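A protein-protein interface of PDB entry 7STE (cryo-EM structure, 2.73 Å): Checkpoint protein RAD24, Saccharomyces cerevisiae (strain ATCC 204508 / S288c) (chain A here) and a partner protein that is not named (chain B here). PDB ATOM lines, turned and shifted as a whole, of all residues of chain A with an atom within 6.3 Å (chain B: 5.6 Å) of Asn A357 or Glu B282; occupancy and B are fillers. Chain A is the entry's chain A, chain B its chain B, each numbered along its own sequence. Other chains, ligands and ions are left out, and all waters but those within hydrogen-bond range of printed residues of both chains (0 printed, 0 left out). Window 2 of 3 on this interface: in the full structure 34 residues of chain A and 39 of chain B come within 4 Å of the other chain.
The guanidinium group (NH2) of Arg A422 sits at hydrogen-bond distance from the side-chain amide oxygen (OD1) of Asn A361 (3.4 Å). The side-chain amide nitrogen (ND2) of Asn A361 lies within hydrogen-bond range of the side-chain amide oxygen (OD1) of Asn A357. The guanidinium group (NH1) of Arg A422 lies within hydrogen-bond range of the side-chain amide oxygen (OD1) of Asn A357 (3.0 Å). The side-chain carboxylate (OE2) of Glu B282 lies within salt-bridge range of the guanidinium group (NH1) of Arg B285 (2.9 Å).
Among the printed residues, merely in contact across the chains: Asn A357 with Lys B275 (3.7 Å), Asn A357 with Leu B277 (3.9 Å), Asn A357 with Glu B282 (3.5 Å), Asn A361 with Lys B275 (3.5 Å), Arg A422 with Arg B285 (3.4 Å), Arg A422 with Leu B286 (3.5 Å) and Lys A426 with Ser B283 (3.9 Å).
Hydrophobic or aromatic side chains of chain B within 4 Å of the printed part of chain A: Leu B286. Among the printed residues, 9 pairs touch across the chains.
Of chain B, only Lys B275, Leu B277, Glu B282 and Arg B285 come within 4 Å of Asn A357. Of the printed residues of chain B, Asn A361 touches Lys B275. Of the printed residues of chain B, Lys A426 touches Ser B283 (3.9 Å). Of the printed residues of chain A, Lys B275 touches Asn A357 and Asn A361. Glu B282 touches just these residues of chain A: Asn A357 (3.5 Å) and Arg A422 (3.9 Å). Printed residues of chain A within 4 Å of Ser B283: Lys A426 (3.9 Å). Of the printed residues of chain A, Leu B286 touches Arg A422 (3.5 Å). The nearest residue of chain A that does not touch Glu B282 is Asp A356 (4.3 Å).
The guanidinium group (NH2) of Arg B285 sits close to the side-chain amide nitrogen (ND2) of Asn A357, at 3.1 Å. The guanidinium group of Arg A422 lies within salt-bridge range of the side-chain carboxylate of Glu B282.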
ATOM      1  N   ASN A 355       6.578  -7.229 -18.911  1.00  0.00           N
ATOM      2  CA  ASN A 355       7.525  -6.122 -18.881  1.00  0.00           C
ATOM      3  C   ASN A 355       8.823  -6.591 -18.233  1.00  0.00           C
ATOM      4  O   ASN A 355       8.824  -7.027 -17.076  1.00  0.00           O
ATOM      5  CB  ASN A 355       6.941  -4.933 -18.119  1.00  0.00           C
ATOM      6  CG  ASN A 355       7.670  -3.636 -18.412  1.00  0.00           C
ATOM      7  OD1 ASN A 355       8.167  -2.973 -17.503  1.00  0.00           O
ATOM      8  ND2 ASN A 355       7.732  -3.266 -19.686  1.00  0.00           N
ATOM      9  N   ASP A 356       9.926  -6.499 -18.979  1.00  0.00           N
ATOM     10  CA  ASP A 356      11.213  -6.938 -18.450  1.00  0.00           C
ATOM     11  C   ASP A 356      11.648  -6.083 -17.267  1.00  0.00           C
ATOM     12  O   ASP A 356      12.151  -6.606 -16.266  1.00  0.00           O
ATOM     13  CB  ASP A 356      12.271  -6.900 -19.553  1.00  0.00           C
ATOM     14  CG  ASP A 356      12.089  -8.006 -20.575  1.00  0.00           C
ATOM     15  OD1 ASP A 356      11.217  -8.874 -20.367  1.00  0.00           O
ATOM     16  OD2 ASP A 356      12.821  -8.005 -21.588  1.00  0.00           O
ATOM     17  N   ASN A 357      11.466  -4.764 -17.364  1.00  0.00           N
ATOM     18  CA  ASN A 357      11.911  -3.879 -16.292  1.00  0.00           C
ATOM     19  C   ASN A 357      11.182  -4.179 -14.988  1.00  0.00           C
ATOM     20  O   ASN A 357      11.804  -4.232 -13.919  1.00  0.00           O
ATOM     21  CB  ASN A 357      11.698  -2.420 -16.695  1.00  0.00           C
ATOM     22  CG  ASN A 357      12.364  -1.449 -15.740  1.00  0.00           C
ATOM     23  OD1 ASN A 357      13.317  -1.801 -15.044  1.00  0.00           O
ATOM     24  ND2 ASN A 357      11.859  -0.223 -15.694  1.00  0.00           N
ATOM     25  N   GLU A 358       9.863  -4.370 -15.054  1.00  0.00           N
ATOM     26  CA  GLU A 358       9.098  -4.656 -13.845  1.00  0.00           C
ATOM     27  C   GLU A 358       9.554  -5.962 -13.208  1.00  0.00           C
ATOM     28  O   GLU A 358       9.736  -6.041 -11.988  1.00  0.00           O
ATOM     29  CB  GLU A 358       7.605  -4.710 -14.174  1.00  0.00           C
ATOM     30  CG  GLU A 358       6.708  -4.847 -12.954  1.00  0.00           C
ATOM     31  CD  GLU A 358       5.233  -4.789 -13.303  1.00  0.00           C
ATOM     32  OE1 GLU A 358       4.901  -4.318 -14.411  1.00  0.00           O
ATOM     33  OE2 GLU A 358       4.406  -5.217 -12.470  1.00  0.00           O
ATOM     34  N   MET A 359       9.743  -7.002 -14.024  1.00  0.00           N
ATOM     35  CA  MET A 359      10.183  -8.286 -13.492  1.00  0.00           C
ATOM     36  C   MET A 359      11.560  -8.163 -12.849  1.00  0.00           C
ATOM     37  O   MET A 359      11.791  -8.694 -11.757  1.00  0.00           O
ATOM     38  CB  MET A 359      10.193  -9.334 -14.607  1.00  0.00           C
ATOM     39  CG  MET A 359      10.784 -10.693 -14.226  1.00  0.00           C
ATOM     40  SD  MET A 359      11.706 -11.453 -15.576  1.00  0.00           S
ATOM     41  CE  MET A 359      13.362 -10.870 -15.228  1.00  0.00           C
ATOM     42  N   ILE A 360      12.484  -7.464 -13.510  1.00  0.00           N
ATOM     43  CA  ILE A 360      13.831  -7.311 -12.965  1.00  0.00           C
ATOM     44  C   ILE A 360      13.782  -6.569 -11.636  1.00  0.00           C
ATOM     45  O   ILE A 360      14.413  -6.977 -10.652  1.00  0.00           O
ATOM     46  CB  ILE A 360      14.739  -6.589 -13.979  1.00  0.00           C
ATOM     47  CG1 ILE A 360      14.990  -7.468 -15.210  1.00  0.00           C
ATOM     48  CG2 ILE A 360      16.058  -6.200 -13.330  1.00  0.00           C
ATOM     49  CD1 ILE A 360      15.844  -8.697 -14.944  1.00  0.00           C
ATOM     50  N   ASN A 361      13.033  -5.465 -11.588  1.00  0.00           N
ATOM     51  CA  ASN A 361      12.962  -4.679 -10.362  1.00  0.00           C
ATOM     52  C   ASN A 361      12.334  -5.482  -9.229  1.00  0.00           C
ATOM     53  O   ASN A 361      12.823  -5.452  -8.093  1.00  0.00           O
ATOM     54  CB  ASN A 361      12.173  -3.394 -10.609  1.00  0.00           C
ATOM     55  CG  ASN A 361      12.934  -2.400 -11.465  1.00  0.00           C
ATOM     56  OD1 ASN A 361      14.156  -2.288 -11.370  1.00  0.00           O
ATOM     57  ND2 ASN A 361      12.213  -1.671 -12.310  1.00  0.00           N
ATOM     58  N   ASN A 362      11.250  -6.206  -9.517  1.00  0.00           N
ATOM     59  CA  ASN A 362      10.601  -6.999  -8.478  1.00  0.00           C
ATOM     60  C   ASN A 362      11.520  -8.106  -7.979  1.00  0.00           C
ATOM     61  O   ASN A 362      11.600  -8.356  -6.770  1.00  0.00           O
ATOM     62  CB  ASN A 362       9.294  -7.586  -9.010  1.00  0.00           C
ATOM     63  CG  ASN A 362       8.269  -6.520  -9.342  1.00  0.00           C
ATOM     64  OD1 ASN A 362       8.481  -5.335  -9.081  1.00  0.00           O
ATOM     65  ND2 ASN A 362       7.149  -6.934  -9.923  1.00  0.00           N
ATOM     66  N   ARG A 422      19.952  -7.602 -17.303  1.00  0.00           N
ATOM     67  CA  ARG A 422      19.201  -6.936 -18.363  1.00  0.00           C
ATOM     68  C   ARG A 422      19.716  -7.337 -19.746  1.00  0.00           C
ATOM     69  O   ARG A 422      18.919  -7.598 -20.655  1.00  0.00           O
ATOM     70  CB  ARG A 422      19.247  -5.422 -18.153  1.00  0.00           C
ATOM     71  CG  ARG A 422      18.452  -4.968 -16.922  1.00  0.00           C
ATOM     72  CD  ARG A 422      18.658  -3.499 -16.595  1.00  0.00           C
ATOM     73  NE  ARG A 422      18.015  -3.130 -15.337  1.00  0.00           N
ATOM     74  CZ  ARG A 422      16.720  -2.880 -15.193  1.00  0.00           C
ATOM     75  NH1 ARG A 422      15.880  -2.968 -16.212  1.00  0.00           N
ATOM     76  NH2 ARG A 422      16.255  -2.541 -13.995  1.00  0.00           N
ATOM     77  N   LYS A 426      17.308  -9.323 -22.347  1.00  0.00           N
ATOM     78  CA  LYS A 426      17.077  -8.719 -23.655  1.00  0.00           C
ATOM     79  C   LYS A 426      17.567  -9.631 -24.773  1.00  0.00           C
ATOM     80  O   LYS A 426      16.884  -9.799 -25.790  1.00  0.00           O
ATOM     81  CB  LYS A 426      17.769  -7.357 -23.722  1.00  0.00           C
ATOM     82  CG  LYS A 426      17.557  -6.598 -25.027  1.00  0.00           C
ATOM     83  CD  LYS A 426      18.799  -5.819 -25.434  1.00  0.00           C
ATOM     84  CE  LYS A 426      19.883  -6.729 -25.990  1.00  0.00           C
ATOM     85  NZ  LYS A 426      21.124  -5.975 -26.313  1.00  0.00           N
ATOM     86  N   LYS B 275      16.998   3.321 -12.719  1.00  0.00           N
ATOM     87  CA  LYS B 275      16.316   2.077 -12.376  1.00  0.00           C
ATOM     88  C   LYS B 275      14.820   2.161 -12.651  1.00  0.00           C
ATOM     89  O   LYS B 275      14.192   1.143 -12.966  1.00  0.00           O
ATOM     90  CB  LYS B 275      16.559   1.731 -10.906  1.00  0.00           C
ATOM     91  CG  LYS B 275      17.918   1.110 -10.632  1.00  0.00           C
ATOM     92  CD  LYS B 275      18.145   0.910  -9.142  1.00  0.00           C
ATOM     93  CE  LYS B 275      17.361  -0.281  -8.615  1.00  0.00           C
ATOM     94  NZ  LYS B 275      17.685  -0.577  -7.193  1.00  0.00           N
ATOM     95  N   ASN B 276      14.233   3.353 -12.542  1.00  0.00           N
ATOM     96  CA  ASN B 276      12.797   3.560 -12.740  1.00  0.00           C
ATOM     97  C   ASN B 276      12.604   4.643 -13.799  1.00  0.00           C
ATOM     98  O   ASN B 276      12.704   5.837 -13.507  1.00  0.00           O
ATOM     99  CB  ASN B 276      12.115   3.929 -11.426  1.00  0.00           C
ATOM    100  CG  ASN B 276      12.652   3.140 -10.248  1.00  0.00           C
ATOM    101  OD1 ASN B 276      13.406   3.662  -9.427  1.00  0.00           O
ATOM    102  ND2 ASN B 276      12.268   1.872 -10.161  1.00  0.00           N
ATOM    103  N   LEU B 277      12.328   4.219 -15.031  1.00  0.00           N
ATOM    104  CA  LEU B 277      12.027   5.125 -16.128  1.00  0.00           C
ATOM    105  C   LEU B 277      10.951   4.488 -16.998  1.00  0.00           C
ATOM    106  O   LEU B 277      10.679   3.288 -16.902  1.00  0.00           O
ATOM    107  CB  LEU B 277      13.280   5.450 -16.954  1.00  0.00           C
ATOM    108  CG  LEU B 277      14.234   6.482 -16.347  1.00  0.00           C
ATOM    109  CD1 LEU B 277      15.505   6.586 -17.176  1.00  0.00           C
ATOM    110  CD2 LEU B 277      13.565   7.844 -16.224  1.00  0.00           C
ATOM    111  N   VAL B 280      12.466   5.222 -21.790  1.00  0.00           N
ATOM    112  CA  VAL B 280      13.730   4.628 -22.202  1.00  0.00           C
ATOM    113  C   VAL B 280      13.532   3.154 -22.522  1.00  0.00           C
ATOM    114  O   VAL B 280      12.870   2.415 -21.779  1.00  0.00           O
ATOM    115  CB  VAL B 280      14.800   4.818 -21.113  1.00  0.00           C
ATOM    116  CG1 VAL B 280      15.062   6.298 -20.880  1.00  0.00           C
ATOM    117  CG2 VAL B 280      14.386   4.125 -19.820  1.00  0.00           C
ATOM    118  N   LYS B 281      14.108   2.718 -23.639  1.00  0.00           N
ATOM    119  CA  LYS B 281      14.059   1.315 -24.012  1.00  0.00           C
ATOM    120  C   LYS B 281      14.909   0.486 -23.054  1.00  0.00           C
ATOM    121  O   LYS B 281      15.808   0.995 -22.377  1.00  0.00           O
ATOM    122  CB  LYS B 281      14.546   1.129 -25.451  1.00  0.00           C
ATOM    123  CG  LYS B 281      14.144  -0.193 -26.090  1.00  0.00           C
ATOM    124  CD  LYS B 281      14.857  -0.411 -27.415  1.00  0.00           C
ATOM    125  CE  LYS B 281      14.684  -1.838 -27.912  1.00  0.00           C
ATOM    126  NZ  LYS B 281      15.499  -2.111 -29.129  1.00  0.00           N
ATOM    127  N   GLU B 282      14.614  -0.814 -23.000  1.00  0.00           N
ATOM    128  CA  GLU B 282      15.355  -1.697 -22.106  1.00  0.00           C
ATOM    129  C   GLU B 282      16.841  -1.695 -22.443  1.00  0.00           C
ATOM    130  O   GLU B 282      17.689  -1.641 -21.544  1.00  0.00           O
ATOM    131  CB  GLU B 282      14.788  -3.114 -22.180  1.00  0.00           C
ATOM    132  CG  GLU B 282      13.312  -3.213 -21.820  1.00  0.00           C
ATOM    133  CD  GLU B 282      13.013  -2.699 -20.424  1.00  0.00           C
ATOM    134  OE1 GLU B 282      13.871  -2.867 -19.532  1.00  0.00           O
ATOM    135  OE2 GLU B 282      11.921  -2.130 -20.219  1.00  0.00           O
ATOM    136  N   SER B 283      17.176  -1.744 -23.734  1.00  0.00           N
ATOM    137  CA  SER B 283      18.579  -1.702 -24.135  1.00  0.00           C
ATOM    138  C   SER B 283      19.229  -0.393 -23.704  1.00  0.00           C
ATOM    139  O   SER B 283      20.341  -0.384 -23.165  1.00  0.00           O
ATOM    140  CB  SER B 283      18.694  -1.889 -25.649  1.00  0.00           C
ATOM    141  OG  SER B 283      20.041  -1.781 -26.076  1.00  0.00           O
ATOM    142  N   VAL B 284      18.541   0.729 -23.926  1.00  0.00           N
ATOM    143  CA  VAL B 284      19.084   2.023 -23.523  1.00  0.00           C
ATOM    144  C   VAL B 284      19.194   2.106 -22.006  1.00  0.00           C
ATOM    145  O   VAL B 284      20.186   2.614 -21.467  1.00  0.00           O
ATOM    146  CB  VAL B 284      18.219   3.164 -24.093  1.00  0.00           C
ATOM    147  CG1 VAL B 284      18.747   4.514 -23.635  1.00  0.00           C
ATOM    148  CG2 VAL B 284      18.178   3.091 -25.612  1.00  0.00           C
ATOM    149  N   ARG B 285      18.179   1.613 -21.294  1.00  0.00           N
ATOM    150  CA  ARG B 285      18.208   1.643 -19.835  1.00  0.00           C
ATOM    151  C   ARG B 285      19.411   0.878 -19.301  1.00  0.00           C
ATOM    152  O   ARG B 285      20.145   1.367 -18.436  1.00  0.00           O
ATOM    153  CB  ARG B 285      16.915   1.047 -19.280  1.00  0.00           C
ATOM    154  CG  ARG B 285      16.862   0.948 -17.762  1.00  0.00           C
ATOM    155  CD  ARG B 285      15.603   0.233 -17.303  1.00  0.00           C
ATOM    156  NE  ARG B 285      14.460   1.136 -17.218  1.00  0.00           N
ATOM    157  CZ  ARG B 285      13.381   1.075 -17.990  1.00  0.00           C
ATOM    158  NH1 ARG B 285      13.258   0.165 -18.946  1.00  0.00           N
ATOM    159  NH2 ARG B 285      12.401   1.949 -17.800  1.00  0.00           N
ATOM    160  N   LEU B 286      19.631  -0.331 -19.817  1.00  0.00           N
ATOM    161  CA  LEU B 286      20.725  -1.156 -19.320  1.00  0.00           C
ATOM    162  C   LEU B 286      22.086  -0.627 -19.764  1.00  0.00           C
ATOM    163  O   LEU B 286      23.064  -0.760 -19.023  1.00  0.00           O
ATOM    164  CB  LEU B 286      20.500  -2.608 -19.751  1.00  0.00           C
ATOM    165  CG  LEU B 286      20.429  -2.883 -21.256  1.00  0.00           C
ATOM    166  CD1 LEU B 286      21.796  -3.028 -21.851  1.00  0.00           C
ATOM    167  CD2 LEU B 286      19.614  -4.139 -21.537  1.00  0.00           C
ATOM    168  N   GLU B 287      22.175   0.003 -20.941  1.00  0.00           N
ATOM    169  CA  GLU B 287      23.427   0.650 -21.323  1.00  0.00           C
ATOM    170  C   GLU B 287      23.740   1.817 -20.393  1.00  0.00           C
ATOM    171  O   GLU B 287      24.894   2.007 -19.983  1.00  0.00           O
ATOM    172  CB  GLU B 287      23.358   1.127 -22.775  1.00  0.00           C
ATOM    173  CG  GLU B 287      23.307   0.012 -23.808  1.00  0.00           C
ATOM    174  CD  GLU B 287      24.670  -0.595 -24.083  1.00  0.00           C
ATOM    175  OE1 GLU B 287      25.654  -0.167 -23.443  1.00  0.00           O
ATOM    176  OE2 GLU B 287      24.759  -1.498 -24.941  1.00  0.00           O
